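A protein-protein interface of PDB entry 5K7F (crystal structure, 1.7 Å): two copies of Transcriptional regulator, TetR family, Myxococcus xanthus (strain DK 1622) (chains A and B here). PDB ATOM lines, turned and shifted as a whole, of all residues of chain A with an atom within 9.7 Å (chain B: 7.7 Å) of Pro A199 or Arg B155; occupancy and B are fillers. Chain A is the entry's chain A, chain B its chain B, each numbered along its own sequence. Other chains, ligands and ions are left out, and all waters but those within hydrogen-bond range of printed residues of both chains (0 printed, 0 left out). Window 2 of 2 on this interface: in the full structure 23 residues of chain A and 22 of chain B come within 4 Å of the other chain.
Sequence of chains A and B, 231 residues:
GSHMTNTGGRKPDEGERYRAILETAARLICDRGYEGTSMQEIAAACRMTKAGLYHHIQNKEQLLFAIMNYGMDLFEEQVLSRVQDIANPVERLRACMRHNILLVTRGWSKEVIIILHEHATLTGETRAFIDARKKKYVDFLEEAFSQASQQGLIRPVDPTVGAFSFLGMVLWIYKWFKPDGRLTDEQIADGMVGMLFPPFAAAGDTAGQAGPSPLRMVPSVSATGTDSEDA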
ATOM      1  N   VAL A  90     -21.207 -19.068 -38.207  1.00  0.00           N
ATOM      2  CA  VAL A  90     -21.772 -18.165 -37.211  1.00  0.00           C
ATOM      3  C   VAL A  90     -22.726 -17.162 -37.857  1.00  0.00           C
ATOM      4  O   VAL A  90     -23.800 -16.882 -37.304  1.00  0.00           O
ATOM      5  CB  VAL A  90     -20.673 -17.481 -36.370  1.00  0.00           C
ATOM      6  CG1 VAL A  90     -20.042 -16.294 -37.036  1.00  0.00           C
ATOM      7  CG2 VAL A  90     -21.279 -17.073 -35.011  1.00  0.00           C
ATOM      8  N   ARG A  94     -26.645 -16.841 -36.800  1.00  0.00           N
ATOM      9  CA  ARG A  94     -27.237 -15.547 -36.455  1.00  0.00           C
ATOM     10  C   ARG A  94     -28.468 -15.249 -37.320  1.00  0.00           C
ATOM     11  O   ARG A  94     -29.506 -14.790 -36.814  1.00  0.00           O
ATOM     12  CB  ARG A  94     -26.217 -14.423 -36.644  1.00  0.00           C
ATOM     13  CG  ARG A  94     -25.091 -14.447 -35.664  1.00  0.00           C
ATOM     14  CD  ARG A  94     -24.102 -13.298 -35.898  1.00  0.00           C
ATOM     15  NE  ARG A  94     -22.965 -13.392 -35.002  1.00  0.00           N
ATOM     16  CZ  ARG A  94     -21.697 -13.166 -35.353  1.00  0.00           C
ATOM     17  NH1 ARG A  94     -21.392 -12.820 -36.599  1.00  0.00           N
ATOM     18  NH2 ARG A  94     -20.735 -13.303 -34.452  1.00  0.00           N
ATOM     19  N   GLY A 152     -13.393 -21.540 -34.558  1.00  0.00           N
ATOM     20  CA  GLY A 152     -13.156 -20.492 -33.582  1.00  0.00           C
ATOM     21  C   GLY A 152     -14.012 -19.255 -33.757  1.00  0.00           C
ATOM     22  O   GLY A 152     -13.605 -18.168 -33.330  1.00  0.00           O
ATOM     23  N   LEU A 153     -15.190 -19.382 -34.383  1.00  0.00           N
ATOM     24  CA  LEU A 153     -16.101 -18.248 -34.527  1.00  0.00           C
ATOM     25  C   LEU A 153     -17.138 -18.168 -33.404  1.00  0.00           C
ATOM     26  O   LEU A 153     -17.822 -17.150 -33.297  1.00  0.00           O
ATOM     27  CB  LEU A 153     -16.799 -18.316 -35.891  1.00  0.00           C
ATOM     28  CG  LEU A 153     -15.872 -18.343 -37.114  1.00  0.00           C
ATOM     29  CD1 LEU A 153     -16.645 -18.853 -38.316  1.00  0.00           C
ATOM     30  CD2 LEU A 153     -15.260 -16.962 -37.417  1.00  0.00           C
ATOM     31  N   ILE A 154     -17.242 -19.202 -32.561  1.00  0.00           N
ATOM     32  CA  ILE A 154     -18.032 -19.183 -31.337  1.00  0.00           C
ATOM     33  C   ILE A 154     -17.212 -19.925 -30.289  1.00  0.00           C
ATOM     34  O   ILE A 154     -16.343 -20.748 -30.608  1.00  0.00           O
ATOM     35  CB  ILE A 154     -19.442 -19.833 -31.457  1.00  0.00           C
ATOM     36  CG1 ILE A 154     -19.331 -21.280 -31.912  1.00  0.00           C
ATOM     37  CG2 ILE A 154     -20.342 -19.047 -32.435  1.00  0.00           C
ATOM     38  CD1 ILE A 154     -20.637 -21.981 -32.056  1.00  0.00           C
ATOM     39  N   ARG A 155     -17.474 -19.597 -29.047  1.00  0.00           N
ATOM     40  CA  ARG A 155     -16.874 -20.330 -27.930  1.00  0.00           C
ATOM     41  C   ARG A 155     -17.234 -21.812 -28.024  1.00  0.00           C
ATOM     42  O   ARG A 155     -18.361 -22.147 -28.406  1.00  0.00           O
ATOM     43  CB  ARG A 155     -17.383 -19.725 -26.620  1.00  0.00           C
ATOM     44  CG  ARG A 155     -16.883 -20.378 -25.359  1.00  0.00           C
ATOM     45  CD  ARG A 155     -17.338 -19.588 -24.118  1.00  0.00           C
ATOM     46  NE  ARG A 155     -17.270 -18.142 -24.339  1.00  0.00           N
ATOM     47  CZ  ARG A 155     -16.223 -17.371 -24.054  1.00  0.00           C
ATOM     48  NH1 ARG A 155     -15.123 -17.895 -23.515  1.00  0.00           N
ATOM     49  NH2 ARG A 155     -16.281 -16.064 -24.311  1.00  0.00           N
ATOM     50  N   ASP A 190     -32.325  -8.996 -31.760  1.00  0.00           N
ATOM     51  CA  ASP A 190     -31.012  -8.374 -31.662  1.00  0.00           C
ATOM     52  C   ASP A 190     -30.327  -8.839 -30.384  1.00  0.00           C
ATOM     53  O   ASP A 190     -29.120  -9.124 -30.375  1.00  0.00           O
ATOM     54  CB  ASP A 190     -31.135  -6.844 -31.691  1.00  0.00           C
ATOM     55  CG  ASP A 190     -31.386  -6.289 -33.086  1.00  0.00           C
ATOM     56  OD1 ASP A 190     -31.176  -6.996 -34.088  1.00  0.00           O
ATOM     57  OD2 ASP A 190     -31.776  -5.109 -33.170  1.00  0.00           O
ATOM     58  N   GLY A 191     -31.094  -8.938 -29.307  1.00  0.00           N
ATOM     59  CA  GLY A 191     -30.554  -9.273 -28.006  1.00  0.00           C
ATOM     60  C   GLY A 191     -30.167 -10.730 -27.868  1.00  0.00           C
ATOM     61  O   GLY A 191     -29.119 -11.051 -27.278  1.00  0.00           O
ATOM     62  N   MET A 192     -31.023 -11.624 -28.381  1.00  0.00           N
ATOM     63  CA  MET A 192     -30.750 -13.062 -28.282  1.00  0.00           C
ATOM     64  C   MET A 192     -29.527 -13.440 -29.104  1.00  0.00           C
ATOM     65  O   MET A 192     -28.671 -14.216 -28.658  1.00  0.00           O
ATOM     66  CB  MET A 192     -31.964 -13.860 -28.739  1.00  0.00           C
ATOM     67  CG  MET A 192     -33.051 -13.955 -27.665  1.00  0.00           C
ATOM     68  SD  MET A 192     -34.339 -15.181 -28.011  1.00  0.00           S
ATOM     69  CE  MET A 192     -35.467 -14.718 -26.731  1.00  0.00           C
ATOM     70  N   VAL A 193     -29.431 -12.899 -30.310  1.00  0.00           N
ATOM     71  CA  VAL A 193     -28.304 -13.200 -31.179  1.00  0.00           C
ATOM     72  C   VAL A 193     -27.039 -12.665 -30.562  1.00  0.00           C
ATOM     73  O   VAL A 193     -25.977 -13.285 -30.652  1.00  0.00           O
ATOM     74  CB  VAL A 193     -28.530 -12.619 -32.595  1.00  0.00           C
ATOM     75  CG1 VAL A 193     -27.263 -12.664 -33.404  1.00  0.00           C
ATOM     76  CG2 VAL A 193     -29.605 -13.422 -33.292  1.00  0.00           C
ATOM     77  N   GLY A 194     -27.135 -11.491 -29.935  1.00  0.00           N
ATOM     78  CA  GLY A 194     -25.974 -10.897 -29.290  1.00  0.00           C
ATOM     79  C   GLY A 194     -25.474 -11.716 -28.119  1.00  0.00           C
ATOM     80  O   GLY A 194     -24.268 -11.732 -27.847  1.00  0.00           O
ATOM     81  N   MET A 195     -26.382 -12.422 -27.439  1.00  0.00           N
ATOM     82  CA  MET A 195     -26.022 -13.285 -26.305  1.00  0.00           C
ATOM     83  C   MET A 195     -25.323 -14.556 -26.758  1.00  0.00           C
ATOM     84  O   MET A 195     -24.298 -14.956 -26.187  1.00  0.00           O
ATOM     85  CB  MET A 195     -27.261 -13.698 -25.518  1.00  0.00           C
ATOM     86  CG  MET A 195     -27.906 -12.655 -24.718  1.00  0.00           C
ATOM     87  SD  MET A 195     -28.866 -13.469 -23.406  1.00  0.00           S
ATOM     88  CE  MET A 195     -27.632 -13.659 -22.208  1.00  0.00           C
ATOM     89  N   LEU A 196     -25.921 -15.267 -27.715  1.00  0.00           N
ATOM     90  CA  LEU A 196     -25.376 -16.557 -28.104  1.00  0.00           C
ATOM     91  C   LEU A 196     -24.243 -16.436 -29.098  1.00  0.00           C
ATOM     92  O   LEU A 196     -23.313 -17.256 -29.070  1.00  0.00           O
ATOM     93  CB  LEU A 196     -26.473 -17.436 -28.703  1.00  0.00           C
ATOM     94  CG  LEU A 196     -27.300 -18.332 -27.783  1.00  0.00           C
ATOM     95  CD1 LEU A 196     -27.762 -19.560 -28.551  1.00  0.00           C
ATOM     96  CD2 LEU A 196     -26.589 -18.758 -26.488  1.00  0.00           C
ATOM     97  N   PHE A 197     -24.294 -15.448 -29.987  1.00  0.00           N
ATOM     98  CA  PHE A 197     -23.363 -15.353 -31.107  1.00  0.00           C
ATOM     99  C   PHE A 197     -22.729 -13.966 -31.183  1.00  0.00           C
ATOM    100  O   PHE A 197     -22.784 -13.299 -32.214  1.00  0.00           O
ATOM    101  CB  PHE A 197     -24.088 -15.686 -32.410  1.00  0.00           C
ATOM    102  CG  PHE A 197     -24.907 -16.957 -32.358  1.00  0.00           C
ATOM    103  CD1 PHE A 197     -24.308 -18.181 -32.157  1.00  0.00           C
ATOM    104  CD2 PHE A 197     -26.283 -16.928 -32.508  1.00  0.00           C
ATOM    105  CE1 PHE A 197     -25.053 -19.339 -32.106  1.00  0.00           C
ATOM    106  CE2 PHE A 197     -27.031 -18.084 -32.492  1.00  0.00           C
ATOM    107  CZ  PHE A 197     -26.422 -19.298 -32.278  1.00  0.00           C
ATOM    108  N   PRO A 198     -22.103 -13.504 -30.110  1.00  0.00           N
ATOM    109  CA  PRO A 198     -21.398 -12.226 -30.160  1.00  0.00           C
ATOM    110  C   PRO A 198     -20.156 -12.341 -31.024  1.00  0.00           C
ATOM    111  O   PRO A 198     -19.709 -13.455 -31.337  1.00  0.00           O
ATOM    112  CB  PRO A 198     -21.020 -11.987 -28.696  1.00  0.00           C
ATOM    113  CG  PRO A 198     -20.758 -13.356 -28.201  1.00  0.00           C
ATOM    114  CD  PRO A 198     -21.814 -14.228 -28.876  1.00  0.00           C
ATOM    115  N   PRO A 199     -19.547 -11.226 -31.408  1.00  0.00           N
ATOM    116  CA  PRO A 199     -18.185 -11.293 -31.954  1.00  0.00           C
ATOM    117  C   PRO A 199     -17.259 -12.045 -31.009  1.00  0.00           C
ATOM    118  O   PRO A 199     -17.243 -11.811 -29.792  1.00  0.00           O
ATOM    119  CB  PRO A 199     -17.788  -9.823 -32.100  1.00  0.00           C
ATOM    120  CG  PRO A 199     -19.112  -9.110 -32.291  1.00  0.00           C
ATOM    121  CD  PRO A 199     -20.117  -9.869 -31.483  1.00  0.00           C
ATOM    122  N   PHE A 200     -16.501 -12.977 -31.574  1.00  0.00           N
ATOM    123  CA  PHE A 200     -15.626 -13.833 -30.797  1.00  0.00           C
ATOM    124  C   PHE A 200     -14.378 -14.168 -31.605  1.00  0.00           C
ATOM    125  O   PHE A 200     -14.496 -14.618 -32.739  1.00  0.00           O
ATOM    126  CB  PHE A 200     -16.357 -15.114 -30.384  1.00  0.00           C
ATOM    127  CG  PHE A 200     -15.466 -16.129 -29.718  1.00  0.00           C
ATOM    128  CD1 PHE A 200     -15.068 -15.968 -28.411  1.00  0.00           C
ATOM    129  CD2 PHE A 200     -15.009 -17.229 -30.420  1.00  0.00           C
ATOM    130  CE1 PHE A 200     -14.240 -16.906 -27.817  1.00  0.00           C
ATOM    131  CE2 PHE A 200     -14.193 -18.150 -29.844  1.00  0.00           C
ATOM    132  CZ  PHE A 200     -13.803 -17.995 -28.538  1.00  0.00           C
ATOM    133  N   PHE B 145     -29.473 -10.081 -13.990  1.00  0.00           N
ATOM    134  CA  PHE B 145     -28.923  -9.692 -15.286  1.00  0.00           C
ATOM    135  C   PHE B 145     -28.576  -8.212 -15.301  1.00  0.00           C
ATOM    136  O   PHE B 145     -27.497  -7.832 -15.740  1.00  0.00           O
ATOM    137  CB  PHE B 145     -29.930 -10.025 -16.384  1.00  0.00           C
ATOM    138  CG  PHE B 145     -29.777 -11.412 -16.967  1.00  0.00           C
ATOM    139  CD1 PHE B 145     -28.728 -11.706 -17.817  1.00  0.00           C
ATOM    140  CD2 PHE B 145     -30.701 -12.401 -16.697  1.00  0.00           C
ATOM    141  CE1 PHE B 145     -28.589 -12.973 -18.383  1.00  0.00           C
ATOM    142  CE2 PHE B 145     -30.565 -13.666 -17.261  1.00  0.00           C
ATOM    143  CZ  PHE B 145     -29.516 -13.959 -18.084  1.00  0.00           C
ATOM    144  N   ALA B 148     -25.433  -7.831 -13.099  1.00  0.00           N
ATOM    145  CA  ALA B 148     -24.270  -8.410 -13.775  1.00  0.00           C
ATOM    146  C   ALA B 148     -23.815  -7.566 -14.956  1.00  0.00           C
ATOM    147  O   ALA B 148     -22.614  -7.423 -15.203  1.00  0.00           O
ATOM    148  CB  ALA B 148     -24.595  -9.814 -14.261  1.00  0.00           C
ATOM    149  N   SER B 149     -24.763  -7.062 -15.728  1.00  0.00           N
ATOM    150  CA  SER B 149     -24.429  -6.206 -16.854  1.00  0.00           C
ATOM    151  C   SER B 149     -23.755  -4.929 -16.368  1.00  0.00           C
ATOM    152  O   SER B 149     -22.642  -4.604 -16.795  1.00  0.00           O
ATOM    153  CB  SER B 149     -25.694  -5.922 -17.637  1.00  0.00           C
ATOM    154  OG  SER B 149     -25.408  -5.098 -18.756  1.00  0.00           O
ATOM    155  N   GLN B 150     -24.368  -4.267 -15.381  1.00  0.00           N
ATOM    156  CA  GLN B 150     -23.815  -3.029 -14.838  1.00  0.00           C
ATOM    157  C   GLN B 150     -22.421  -3.218 -14.269  1.00  0.00           C
ATOM    158  O   GLN B 150     -21.604  -2.295 -14.338  1.00  0.00           O
ATOM    159  CB  GLN B 150     -24.715  -2.482 -13.735  1.00  0.00           C
ATOM    160  CG  GLN B 150     -25.816  -1.555 -14.178  1.00  0.00           C
ATOM    161  CD  GLN B 150     -26.432  -0.851 -12.987  1.00  0.00           C
ATOM    162  OE1 GLN B 150     -26.289  -1.309 -11.843  1.00  0.00           O
ATOM    163  NE2 GLN B 150     -27.101   0.275 -13.236  1.00  0.00           N
ATOM    164  N   GLY B 152     -20.159  -5.314 -15.245  1.00  0.00           N
ATOM    165  CA  GLY B 152     -19.182  -5.764 -16.220  1.00  0.00           C
ATOM    166  C   GLY B 152     -18.862  -7.231 -16.112  1.00  0.00           C
ATOM    167  O   GLY B 152     -17.770  -7.647 -16.514  1.00  0.00           O
ATOM    168  N   LEU B 153     -19.784  -8.024 -15.565  1.00  0.00           N
ATOM    169  CA  LEU B 153     -19.558  -9.463 -15.390  1.00  0.00           C
ATOM    170  C   LEU B 153     -20.186 -10.293 -16.496  1.00  0.00           C
ATOM    171  O   LEU B 153     -19.880 -11.493 -16.625  1.00  0.00           O
ATOM    172  CB  LEU B 153     -20.111  -9.925 -14.027  1.00  0.00           C
ATOM    173  CG  LEU B 153     -19.528  -9.247 -12.773  1.00  0.00           C
ATOM    174  CD1 LEU B 153     -20.321  -9.575 -11.512  1.00  0.00           C
ATOM    175  CD2 LEU B 153     -18.081  -9.655 -12.616  1.00  0.00           C
ATOM    176  N   ILE B 154     -21.089  -9.697 -17.256  1.00  0.00           N
ATOM    177  CA  ILE B 154     -21.632 -10.300 -18.466  1.00  0.00           C
ATOM    178  C   ILE B 154     -21.646  -9.244 -19.566  1.00  0.00           C
ATOM    179  O   ILE B 154     -21.672  -8.037 -19.297  1.00  0.00           O
ATOM    180  CB  ILE B 154     -23.054 -10.874 -18.244  1.00  0.00           C
ATOM    181  CG1 ILE B 154     -24.010  -9.796 -17.802  1.00  0.00           C
ATOM    182  CG2 ILE B 154     -23.009 -11.989 -17.216  1.00  0.00           C
ATOM    183  CD1 ILE B 154     -25.455 -10.240 -17.765  1.00  0.00           C
ATOM    184  N   ARG B 155     -21.601  -9.717 -20.818  1.00  0.00           N
ATOM    185  CA  ARG B 155     -21.815  -8.847 -21.965  1.00  0.00           C
ATOM    186  C   ARG B 155     -23.154  -8.135 -21.786  1.00  0.00           C
ATOM    187  O   ARG B 155     -24.132  -8.760 -21.354  1.00  0.00           O
ATOM    188  CB  ARG B 155     -21.792  -9.641 -23.278  1.00  0.00           C
ATOM    189  CG  ARG B 155     -21.837  -8.808 -24.529  1.00  0.00           C
ATOM    190  CD  ARG B 155     -21.740  -9.683 -25.780  1.00  0.00           C
ATOM    191  NE  ARG B 155     -21.864  -8.849 -26.978  1.00  0.00           N
ATOM    192  CZ  ARG B 155     -20.839  -8.256 -27.586  1.00  0.00           C
ATOM    193  NH1 ARG B 155     -19.596  -8.415 -27.137  1.00  0.00           N
ATOM    194  NH2 ARG B 155     -21.062  -7.498 -28.645  1.00  0.00           N
ATOM    195  N   PRO B 156     -23.227  -6.835 -22.026  1.00  0.00           N
ATOM    196  CA  PRO B 156     -24.488  -6.143 -21.785  1.00  0.00           C
ATOM    197  C   PRO B 156     -25.621  -6.793 -22.562  1.00  0.00           C
ATOM    198  O   PRO B 156     -25.447  -7.248 -23.701  1.00  0.00           O
ATOM    199  CB  PRO B 156     -24.200  -4.717 -22.256  1.00  0.00           C
ATOM    200  CG  PRO B 156     -22.733  -4.563 -21.889  1.00  0.00           C
ATOM    201  CD  PRO B 156     -22.116  -5.895 -22.222  1.00  0.00           C
ATOM    202  N   VAL B 157     -26.793  -6.794 -21.933  1.00  0.00           N
ATOM    203  CA  VAL B 157     -28.014  -7.302 -22.547  1.00  0.00           C
ATOM    204  C   VAL B 157     -29.174  -6.672 -21.810  1.00  0.00           C
ATOM    205  O   VAL B 157     -29.040  -6.257 -20.664  1.00  0.00           O
ATOM    206  CB  VAL B 157     -28.079  -8.850 -22.496  1.00  0.00           C
ATOM    207  CG1 VAL B 157     -28.149  -9.398 -21.027  1.00  0.00           C
ATOM    208  CG2 VAL B 157     -29.249  -9.331 -23.336  1.00  0.00           C
ATOM    209  N   ASP B 158     -30.310  -6.593 -22.473  1.00  0.00           N
ATOM    210  CA  ASP B 158     -31.524  -6.154 -21.816  1.00  0.00           C
ATOM    211  C   ASP B 158     -31.907  -7.203 -20.780  1.00  0.00           C
ATOM    212  O   ASP B 158     -31.885  -8.401 -21.105  1.00  0.00           O
ATOM    213  CB  ASP B 158     -32.630  -5.970 -22.841  1.00  0.00           C
ATOM    214  CG  ASP B 158     -33.905  -5.468 -22.234  1.00  0.00           C
ATOM    215  OD1 ASP B 158     -34.575  -6.208 -21.486  1.00  0.00           O
ATOM    216  OD2 ASP B 158     -34.251  -4.296 -22.499  1.00  0.00           O
ATOM    217  N   LEU B 196     -24.284 -18.997 -21.612  1.00  0.00           N
ATOM    218  CA  LEU B 196     -24.823 -17.694 -21.230  1.00  0.00           C
ATOM    219  C   LEU B 196     -23.888 -16.925 -20.318  1.00  0.00           C
ATOM    220  O   LEU B 196     -23.914 -15.692 -20.306  1.00  0.00           O
ATOM    221  CB  LEU B 196     -26.166 -17.830 -20.505  1.00  0.00           C
ATOM    222  CG  LEU B 196     -27.435 -18.161 -21.249  1.00  0.00           C
ATOM    223  CD1 LEU B 196     -28.583 -17.835 -20.334  1.00  0.00           C
ATOM    224  CD2 LEU B 196     -27.536 -17.343 -22.556  1.00  0.00           C
ATOM    225  N   PHE B 197     -23.066 -17.614 -19.547  1.00  0.00           N
ATOM    226  CA  PHE B 197     -22.288 -16.973 -18.479  1.00  0.00           C
ATOM    227  C   PHE B 197     -20.831 -17.402 -18.495  1.00  0.00           C
ATOM    228  O   PHE B 197     -20.313 -17.926 -17.497  1.00  0.00           O
ATOM    229  CB  PHE B 197     -22.898 -17.294 -17.122  1.00  0.00           C
ATOM    230  CG  PHE B 197     -24.363 -17.005 -17.037  1.00  0.00           C
ATOM    231  CD1 PHE B 197     -24.825 -15.691 -17.151  1.00  0.00           C
ATOM    232  CD2 PHE B 197     -25.272 -18.029 -16.842  1.00  0.00           C
ATOM    233  CE1 PHE B 197     -26.170 -15.410 -17.061  1.00  0.00           C
ATOM    234  CE2 PHE B 197     -26.638 -17.767 -16.714  1.00  0.00           C
ATOM    235  CZ  PHE B 197     -27.096 -16.456 -16.850  1.00  0.00           C
ATOM    236  N   PRO B 198     -20.152 -17.228 -19.610  1.00  0.00           N
ATOM    237  CA  PRO B 198     -18.743 -17.553 -19.657  1.00  0.00           C
ATOM    238  C   PRO B 198     -17.947 -16.536 -18.872  1.00  0.00           C
ATOM    239  O   PRO B 198     -18.437 -15.429 -18.602  1.00  0.00           O
ATOM    240  CB  PRO B 198     -18.420 -17.474 -21.145  1.00  0.00           C
ATOM    241  CG  PRO B 198     -19.263 -16.366 -21.614  1.00  0.00           C
ATOM    242  CD  PRO B 198     -20.573 -16.521 -20.825  1.00  0.00           C
ATOM    243  N   PHE B 200     -16.026 -13.478 -18.330  1.00  0.00           N
ATOM    244  CA  PHE B 200     -16.137 -12.243 -19.093  1.00  0.00           C
ATOM    245  C   PHE B 200     -15.477 -11.094 -18.339  1.00  0.00           C
ATOM    246  O   PHE B 200     -14.758 -10.305 -18.946  1.00  0.00           O
ATOM    247  CB  PHE B 200     -17.605 -11.915 -19.373  1.00  0.00           C
ATOM    248  CG  PHE B 200     -17.807 -10.616 -20.124  1.00  0.00           C
ATOM    249  CD1 PHE B 200     -17.978  -9.420 -19.436  1.00  0.00           C
ATOM    250  CD2 PHE B 200     -17.838 -10.593 -21.508  1.00  0.00           C
ATOM    251  CE1 PHE B 200     -18.162  -8.235 -20.112  1.00  0.00           C
ATOM    252  CE2 PHE B 200     -18.024  -9.408 -22.186  1.00  0.00           C
ATOM    253  CZ  PHE B 200     -18.188  -8.226 -21.480  1.00  0.00           C
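O of Pro A198 is in hydrogen-bond range of NH2 of Arg A94, at 3.3 Å.
Arg A155 touches Pro B198.
Arg B155 touches Gly A194.
CG of Met A195 touches CG2 of Val B157, 3.8 Å away.
Met A195 touches Leu B196 (CE to CD2, 3.7 Å).
Pro A198 touches Arg B155.
CD of Pro A199 touches NH2 of Arg B155, 3.8 Å away.
Pro A199 touches one residue of chain B.
Arg B155 touches just these residues of chain A: Gly A194, Pro A198 and Pro A199.
No residue of chain A comes within 4 Å of Pro B156.
Val B157 touches just one residue of chain A: Met A195.
Printed residues of chain B within 4 Å of Gly A194: Arg B155 (3.9 Å).
Printed residues of chain B within 4 Å of Pro A198: Arg B155 (3.7 Å).
Of the printed residues of chain A, Pro B198 touches Arg A155.
Printed residues of chain B within 4 Å of Met A195: Val B157 (3.8 Å) and Leu B196 (3.7 Å).
Phe B200 touches none of the printed residues of chain A.
Gly B152 touches none of the printed residues of chain A.
The nearest residue of chain A that does not touch Arg B155 is Met A195 (5.6 Å).
Printed residues of chain A that touch a printed residue of chain B: Arg A155, Gly A194, Met A195, Pro A198 and Pro A199.
Hydrophobic or aromatic side chains of chain A that line the printed part of chain B: Met A195, Pro A198 and Pro A199.
Of the 15 printed residues of chain B, 4 touch a printed residue of chain A.
Hydrophobic or aromatic side chains of chain B that line the printed part of chain A: Val B157, Leu B196 and Pro B198.
Arg A155 touches Pro B198, and with the chains exchanged Pro A198 touches Arg B155.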
